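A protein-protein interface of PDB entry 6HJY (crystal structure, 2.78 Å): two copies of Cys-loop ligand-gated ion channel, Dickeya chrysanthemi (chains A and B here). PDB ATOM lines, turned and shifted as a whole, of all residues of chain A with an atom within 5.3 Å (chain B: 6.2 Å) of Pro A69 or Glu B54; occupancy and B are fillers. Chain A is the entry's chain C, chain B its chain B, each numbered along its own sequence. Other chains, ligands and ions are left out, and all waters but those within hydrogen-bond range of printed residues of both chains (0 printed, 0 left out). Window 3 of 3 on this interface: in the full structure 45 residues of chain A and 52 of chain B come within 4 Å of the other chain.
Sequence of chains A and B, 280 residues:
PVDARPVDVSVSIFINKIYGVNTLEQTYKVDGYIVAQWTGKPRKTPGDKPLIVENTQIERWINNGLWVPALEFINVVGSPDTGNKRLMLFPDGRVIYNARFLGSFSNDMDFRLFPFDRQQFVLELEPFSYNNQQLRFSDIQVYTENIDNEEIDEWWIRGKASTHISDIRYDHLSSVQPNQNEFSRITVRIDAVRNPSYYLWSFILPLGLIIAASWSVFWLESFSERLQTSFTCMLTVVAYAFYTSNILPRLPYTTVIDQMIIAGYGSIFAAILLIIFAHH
Hydrophobic or aromatic side chains of chain A that line the printed part of chain B: Ala A70, Phe A128 and Tyr A130. Hydrophobic or aromatic side chains of chain B that line the printed part of chain A: Ile B52. Among the printed residues, no Asp or Glu carboxylate lies within 4 Å of a Lys or Arg side-chain nitrogen of the other chain.
Trp A67 touches none of the printed residues of chain B. Printed residues of chain B within 4 Å of Pro A69: Glu B54 (3.9 Å). Of the printed residues of chain B, Ala A70 touches Glu B54, Asn B55 and Asn B84. Of the printed residues of chain B, Phe A128 touches Asn B84 (3.2 Å), Lys B85 (3.8 Å) and Arg B86 (3.7 Å). Printed residues of chain A within 4 Å of Asn B55: Ala A70. Printed residues of chain A within 4 Å of Asn B84: Ala A70 and Phe A128. Leu B87 touches none of the printed residues of chain A. The nearest printed residue of chain A that does not touch Glu B54 is Tyr A130 (4.01 Å).
Pro A69 touches Glu B54. Asn B55 touches Ala A70. CB of Ala A70 touches OD1 of Asn B84, at 3.3 Å. Asn B84 touches Phe A128. Phe A128 touches Lys B85. CE2 of Phe A128 touches CB of Arg B86, at 3.7 Å. Ile B52 touches Ser A129 (CG2 to CB, 3.6 Å). Ser A129 touches Arg B86. OH of Tyr A130 touches CG2 of Ile B52 (3.6 Å).
OE1 of Glu B54 sits at hydrogen-bond distance from N of Ala A70 (3.1 Å). The side-chain carboxylate (OE2) of Glu B54 sits at hydrogen-bond distance from the side-chain hydroxyl (OG) of Ser A129 (2.7 Å).
No position is printed for both chains. Of the 11 pairs that touch across the chains among the printed residues, none has its exchanged pair printed and touching as well.
The side-chain amide nitrogen of Asn B55 sits at hydrogen-bond distance from the side-chain amide oxygen of Asn B84, at 3.1 Å. The backbone NH of Lys B85 lies within hydrogen-bond range of the side-chain amide oxygen of Asn B55, 2.9 Å away. The indole nitrogen (NE1) of Trp A67 sits at hydrogen-bond distance from the side-chain hydroxyl (OH) of Tyr A130. O of Ala A70 lies within hydrogen-bond range of N of Phe A128 (2.9 Å).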
ATOM      1  N   TRP A  38      27.265  22.418 -12.762  1.00  0.00           N
ATOM      2  CA  TRP A  38      27.488  21.235 -13.584  1.00  0.00           C
ATOM      3  C   TRP A  38      27.543  21.619 -15.056  1.00  0.00           C
ATOM      4  O   TRP A  38      27.291  22.777 -15.396  1.00  0.00           O
ATOM      5  CB  TRP A  38      26.411  20.165 -13.325  1.00  0.00           C
ATOM      6  CG  TRP A  38      25.020  20.574 -13.708  1.00  0.00           C
ATOM      7  CD1 TRP A  38      24.387  20.328 -14.890  1.00  0.00           C
ATOM      8  CD2 TRP A  38      24.083  21.289 -12.890  1.00  0.00           C
ATOM      9  NE1 TRP A  38      23.111  20.844 -14.861  1.00  0.00           N
ATOM     10  CE2 TRP A  38      22.898  21.444 -13.645  1.00  0.00           C
ATOM     11  CE3 TRP A  38      24.127  21.817 -11.586  1.00  0.00           C
ATOM     12  CZ2 TRP A  38      21.760  22.087 -13.131  1.00  0.00           C
ATOM     13  CZ3 TRP A  38      23.009  22.470 -11.086  1.00  0.00           C
ATOM     14  CH2 TRP A  38      21.848  22.612 -11.857  1.00  0.00           C
ATOM     15  N   TRP A  67      17.023  20.392 -17.011  1.00  0.00           N
ATOM     16  CA  TRP A  67      17.321  19.543 -15.861  1.00  0.00           C
ATOM     17  C   TRP A  67      17.949  20.327 -14.700  1.00  0.00           C
ATOM     18  O   TRP A  67      19.101  20.766 -14.781  1.00  0.00           O
ATOM     19  CB  TRP A  67      18.192  18.351 -16.293  1.00  0.00           C
ATOM     20  CG  TRP A  67      18.428  17.333 -15.217  1.00  0.00           C
ATOM     21  CD1 TRP A  67      17.555  16.379 -14.783  1.00  0.00           C
ATOM     22  CD2 TRP A  67      19.625  17.163 -14.446  1.00  0.00           C
ATOM     23  NE1 TRP A  67      18.136  15.617 -13.794  1.00  0.00           N
ATOM     24  CE2 TRP A  67      19.407  16.079 -13.564  1.00  0.00           C
ATOM     25  CE3 TRP A  67      20.867  17.823 -14.416  1.00  0.00           C
ATOM     26  CZ2 TRP A  67      20.381  15.644 -12.659  1.00  0.00           C
ATOM     27  CZ3 TRP A  67      21.834  17.387 -13.524  1.00  0.00           C
ATOM     28  CH2 TRP A  67      21.592  16.304 -12.667  1.00  0.00           C
ATOM     29  N   VAL A  68      17.153  20.549 -13.636  1.00  0.00           N
ATOM     30  CA  VAL A  68      17.582  21.260 -12.428  1.00  0.00           C
ATOM     31  C   VAL A  68      17.271  20.303 -11.264  1.00  0.00           C
ATOM     32  O   VAL A  68      16.132  20.272 -10.801  1.00  0.00           O
ATOM     33  CB  VAL A  68      16.924  22.668 -12.253  1.00  0.00           C
ATOM     34  CG1 VAL A  68      17.555  23.424 -11.088  1.00  0.00           C
ATOM     35  CG2 VAL A  68      17.024  23.505 -13.527  1.00  0.00           C
ATOM     36  N   PRO A  69      18.234  19.456 -10.838  1.00  0.00           N
ATOM     37  CA  PRO A  69      17.940  18.507  -9.759  1.00  0.00           C
ATOM     38  C   PRO A  69      17.688  19.177  -8.416  1.00  0.00           C
ATOM     39  O   PRO A  69      18.261  20.223  -8.112  1.00  0.00           O
ATOM     40  CB  PRO A  69      19.200  17.649  -9.705  1.00  0.00           C
ATOM     41  CG  PRO A  69      20.282  18.555 -10.179  1.00  0.00           C
ATOM     42  CD  PRO A  69      19.635  19.335 -11.286  1.00  0.00           C
ATOM     43  N   ALA A  70      16.824  18.556  -7.616  1.00  0.00           N
ATOM     44  CA  ALA A  70      16.512  19.022  -6.280  1.00  0.00           C
ATOM     45  C   ALA A  70      17.531  18.439  -5.327  1.00  0.00           C
ATOM     46  O   ALA A  70      17.734  17.215  -5.287  1.00  0.00           O
ATOM     47  CB  ALA A  70      15.117  18.581  -5.882  1.00  0.00           C
ATOM     48  N   LEU A  71      18.233  19.326  -4.623  1.00  0.00           N
ATOM     49  CA  LEU A  71      19.230  18.944  -3.628  1.00  0.00           C
ATOM     50  C   LEU A  71      18.596  19.189  -2.282  1.00  0.00           C
ATOM     51  O   LEU A  71      17.939  20.211  -2.082  1.00  0.00           O
ATOM     52  CB  LEU A  71      20.546  19.720  -3.809  1.00  0.00           C
ATOM     53  CG  LEU A  71      21.158  19.659  -5.212  1.00  0.00           C
ATOM     54  CD1 LEU A  71      22.143  20.773  -5.422  1.00  0.00           C
ATOM     55  CD2 LEU A  71      21.774  18.284  -5.509  1.00  0.00           C
ATOM     56  N   PHE A 128      17.923  14.674  -3.880  1.00  0.00           N
ATOM     57  CA  PHE A 128      16.699  14.044  -3.397  1.00  0.00           C
ATOM     58  C   PHE A 128      16.302  12.783  -4.158  1.00  0.00           C
ATOM     59  O   PHE A 128      15.741  11.872  -3.549  1.00  0.00           O
ATOM     60  CB  PHE A 128      15.533  15.055  -3.358  1.00  0.00           C
ATOM     61  CG  PHE A 128      14.290  14.525  -2.675  1.00  0.00           C
ATOM     62  CD1 PHE A 128      14.236  14.401  -1.291  1.00  0.00           C
ATOM     63  CD2 PHE A 128      13.186  14.124  -3.417  1.00  0.00           C
ATOM     64  CE1 PHE A 128      13.095  13.898  -0.664  1.00  0.00           C
ATOM     65  CE2 PHE A 128      12.045  13.622  -2.788  1.00  0.00           C
ATOM     66  CZ  PHE A 128      12.010  13.509  -1.419  1.00  0.00           C
ATOM     67  N   SER A 129      16.589  12.720  -5.466  1.00  0.00           N
ATOM     68  CA  SER A 129      16.142  11.625  -6.326  1.00  0.00           C
ATOM     69  C   SER A 129      17.207  10.905  -7.138  1.00  0.00           C
ATOM     70  O   SER A 129      16.996   9.749  -7.519  1.00  0.00           O
ATOM     71  CB  SER A 129      15.097  12.163  -7.289  1.00  0.00           C
ATOM     72  OG  SER A 129      14.113  12.918  -6.603  1.00  0.00           O
ATOM     73  N   TYR A 130      18.314  11.591  -7.452  1.00  0.00           N
ATOM     74  CA  TYR A 130      19.379  11.045  -8.288  1.00  0.00           C
ATOM     75  C   TYR A 130      20.501  10.398  -7.518  1.00  0.00           C
ATOM     76  O   TYR A 130      21.169  11.054  -6.720  1.00  0.00           O
ATOM     77  CB  TYR A 130      19.911  12.126  -9.243  1.00  0.00           C
ATOM     78  CG  TYR A 130      18.821  12.698 -10.127  1.00  0.00           C
ATOM     79  CD1 TYR A 130      18.350  11.987 -11.232  1.00  0.00           C
ATOM     80  CD2 TYR A 130      18.224  13.923  -9.836  1.00  0.00           C
ATOM     81  CE1 TYR A 130      17.314  12.486 -12.024  1.00  0.00           C
ATOM     82  CE2 TYR A 130      17.197  14.435 -10.628  1.00  0.00           C
ATOM     83  CZ  TYR A 130      16.748  13.712 -11.721  1.00  0.00           C
ATOM     84  OH  TYR A 130      15.736  14.209 -12.496  1.00  0.00           O
ATOM     85  N   LEU A 135      24.111  11.382 -10.501  1.00  0.00           N
ATOM     86  CA  LEU A 135      24.591  12.651  -9.958  1.00  0.00           C
ATOM     87  C   LEU A 135      25.507  12.430  -8.768  1.00  0.00           C
ATOM     88  O   LEU A 135      25.088  11.882  -7.745  1.00  0.00           O
ATOM     89  CB  LEU A 135      23.379  13.511  -9.538  1.00  0.00           C
ATOM     90  CG  LEU A 135      23.544  15.027  -9.355  1.00  0.00           C
ATOM     91  CD1 LEU A 135      22.204  15.667  -9.225  1.00  0.00           C
ATOM     92  CD2 LEU A 135      24.349  15.380  -8.094  1.00  0.00           C
ATOM     93  N   ILE B  52      12.255  10.012 -13.378  1.00  0.00           N
ATOM     94  CA  ILE B  52      12.169  10.796 -12.149  1.00  0.00           C
ATOM     95  C   ILE B  52      11.448  12.127 -12.429  1.00  0.00           C
ATOM     96  O   ILE B  52      11.844  12.874 -13.330  1.00  0.00           O
ATOM     97  CB  ILE B  52      13.551  10.958 -11.457  1.00  0.00           C
ATOM     98  CG1 ILE B  52      13.944   9.655 -10.733  1.00  0.00           C
ATOM     99  CG2 ILE B  52      13.560  12.149 -10.490  1.00  0.00           C
ATOM    100  CD1 ILE B  52      15.430   9.338 -10.748  1.00  0.00           C
ATOM    101  N   VAL B  53      10.354  12.379 -11.679  1.00  0.00           N
ATOM    102  CA  VAL B  53       9.520  13.592 -11.748  1.00  0.00           C
ATOM    103  C   VAL B  53       9.559  14.230 -10.336  1.00  0.00           C
ATOM    104  O   VAL B  53       9.155  13.595  -9.361  1.00  0.00           O
ATOM    105  CB  VAL B  53       8.060  13.298 -12.222  1.00  0.00           C
ATOM    106  CG1 VAL B  53       7.327  14.580 -12.549  1.00  0.00           C
ATOM    107  CG2 VAL B  53       8.023  12.372 -13.436  1.00  0.00           C
ATOM    108  N   GLU B  54      10.132  15.441 -10.213  1.00  0.00           N
ATOM    109  CA  GLU B  54      10.251  16.108  -8.918  1.00  0.00           C
ATOM    110  C   GLU B  54       9.329  17.312  -8.762  1.00  0.00           C
ATOM    111  O   GLU B  54       8.954  17.973  -9.728  1.00  0.00           O
ATOM    112  CB  GLU B  54      11.692  16.577  -8.668  1.00  0.00           C
ATOM    113  CG  GLU B  54      12.693  15.485  -8.322  1.00  0.00           C
ATOM    114  CD  GLU B  54      14.134  15.966  -8.247  1.00  0.00           C
ATOM    115  OE1 GLU B  54      14.484  16.932  -8.956  1.00  0.00           O
ATOM    116  OE2 GLU B  54      14.916  15.384  -7.467  1.00  0.00           O
ATOM    117  N   ASN B  55       8.967  17.570  -7.505  1.00  0.00           N
ATOM    118  CA  ASN B  55       8.197  18.659  -6.924  1.00  0.00           C
ATOM    119  C   ASN B  55       7.053  19.227  -7.811  1.00  0.00           C
ATOM    120  O   ASN B  55       6.000  18.593  -7.905  1.00  0.00           O
ATOM    121  CB  ASN B  55       9.144  19.788  -6.490  1.00  0.00           C
ATOM    122  CG  ASN B  55      10.165  19.361  -5.457  1.00  0.00           C
ATOM    123  OD1 ASN B  55       9.830  18.805  -4.418  1.00  0.00           O
ATOM    124  ND2 ASN B  55      11.438  19.598  -5.726  1.00  0.00           N
ATOM    125  N   THR B  56       7.270  20.398  -8.441  1.00  0.00           N
ATOM    126  CA  THR B  56       6.304  21.123  -9.275  1.00  0.00           C
ATOM    127  C   THR B  56       5.956  20.391 -10.583  1.00  0.00           C
ATOM    128  O   THR B  56       4.862  20.607 -11.105  1.00  0.00           O
ATOM    129  CB  THR B  56       6.777  22.562  -9.519  1.00  0.00           C
ATOM    130  OG1 THR B  56       8.194  22.583  -9.666  1.00  0.00           O
ATOM    131  CG2 THR B  56       6.357  23.519  -8.395  1.00  0.00           C
ATOM    132  N   GLN B  57       6.849  19.502 -11.077  1.00  0.00           N
ATOM    133  CA  GLN B  57       6.606  18.707 -12.284  1.00  0.00           C
ATOM    134  C   GLN B  57       5.578  17.592 -12.048  1.00  0.00           C
ATOM    135  O   GLN B  57       4.925  17.184 -13.009  1.00  0.00           O
ATOM    136  CB  GLN B  57       7.916  18.132 -12.863  1.00  0.00           C
ATOM    137  CG  GLN B  57       8.880  19.180 -13.438  1.00  0.00           C
ATOM    138  CD  GLN B  57       8.166  20.073 -14.410  1.00  0.00           C
ATOM    139  OE1 GLN B  57       7.769  19.640 -15.490  1.00  0.00           O
ATOM    140  NE2 GLN B  57       7.837  21.271 -13.968  1.00  0.00           N
ATOM    141  N   ILE B  58       5.428  17.111 -10.774  1.00  0.00           N
ATOM    142  CA  ILE B  58       4.485  16.062 -10.343  1.00  0.00           C
ATOM    143  C   ILE B  58       3.061  16.479 -10.726  1.00  0.00           C
ATOM    144  O   ILE B  58       2.321  15.679 -11.306  1.00  0.00           O
ATOM    145  CB  ILE B  58       4.606  15.735  -8.805  1.00  0.00           C
ATOM    146  CG1 ILE B  58       5.932  14.985  -8.494  1.00  0.00           C
ATOM    147  CG2 ILE B  58       3.365  14.952  -8.266  1.00  0.00           C
ATOM    148  CD1 ILE B  58       6.212  14.596  -7.063  1.00  0.00           C
ATOM    149  N   ASN B  84      10.736  18.289  -0.213  1.00  0.00           N
ATOM    150  CA  ASN B  84      10.831  17.775  -1.580  1.00  0.00           C
ATOM    151  C   ASN B  84       9.948  16.559  -1.746  1.00  0.00           C
ATOM    152  O   ASN B  84       9.794  15.777  -0.807  1.00  0.00           O
ATOM    153  CB  ASN B  84      12.266  17.382  -1.920  1.00  0.00           C
ATOM    154  CG  ASN B  84      13.182  18.540  -2.147  1.00  0.00           C
ATOM    155  OD1 ASN B  84      13.183  19.158  -3.215  1.00  0.00           O
ATOM    156  ND2 ASN B  84      14.010  18.818  -1.158  1.00  0.00           N
ATOM    157  N   LYS B  85       9.368  16.402  -2.934  1.00  0.00           N
ATOM    158  CA  LYS B  85       8.568  15.236  -3.295  1.00  0.00           C
ATOM    159  C   LYS B  85       8.967  14.748  -4.685  1.00  0.00           C
ATOM    160  O   LYS B  85       9.410  15.544  -5.522  1.00  0.00           O
ATOM    161  CB  LYS B  85       7.050  15.425  -3.107  1.00  0.00           C
ATOM    162  CG  LYS B  85       6.392  16.583  -3.845  1.00  0.00           C
ATOM    163  CD  LYS B  85       4.928  16.626  -3.435  1.00  0.00           C
ATOM    164  CE  LYS B  85       4.073  17.560  -4.254  1.00  0.00           C
ATOM    165  NZ  LYS B  85       2.632  17.379  -3.893  1.00  0.00           N
ATOM    166  N   ARG B  86       8.904  13.420  -4.888  1.00  0.00           N
ATOM    167  CA  ARG B  86       9.328  12.773  -6.121  1.00  0.00           C
ATOM    168  C   ARG B  86       8.468  11.581  -6.513  1.00  0.00           C
ATOM    169  O   ARG B  86       8.072  10.779  -5.665  1.00  0.00           O
ATOM    170  CB  ARG B  86      10.802  12.340  -5.989  1.00  0.00           C
ATOM    171  CG  ARG B  86      11.324  11.456  -7.117  1.00  0.00           C
ATOM    172  CD  ARG B  86      12.224  10.343  -6.611  1.00  0.00           C
ATOM    173  NE  ARG B  86      11.492   9.220  -6.035  1.00  0.00           N
ATOM    174  CZ  ARG B  86      12.075   8.107  -5.607  1.00  0.00           C
ATOM    175  NH1 ARG B  86      13.392   7.967  -5.686  1.00  0.00           N
ATOM    176  NH2 ARG B  86      11.346   7.123  -5.094  1.00  0.00           N
ATOM    177  N   LEU B  87       8.249  11.433  -7.827  1.00  0.00           N
ATOM    178  CA  LEU B  87       7.577  10.284  -8.411  1.00  0.00           C
ATOM    179  C   LEU B  87       8.592   9.533  -9.253  1.00  0.00           C
ATOM    180  O   LEU B  87       9.336  10.148 -10.021  1.00  0.00           O
ATOM    181  CB  LEU B  87       6.401  10.701  -9.312  1.00  0.00           C
ATOM    182  CG  LEU B  87       5.071  11.067  -8.660  1.00  0.00           C
ATOM    183  CD1 LEU B  87       4.103  11.555  -9.707  1.00  0.00           C
ATOM    184  CD2 LEU B  87       4.463   9.881  -7.898  1.00  0.00           C
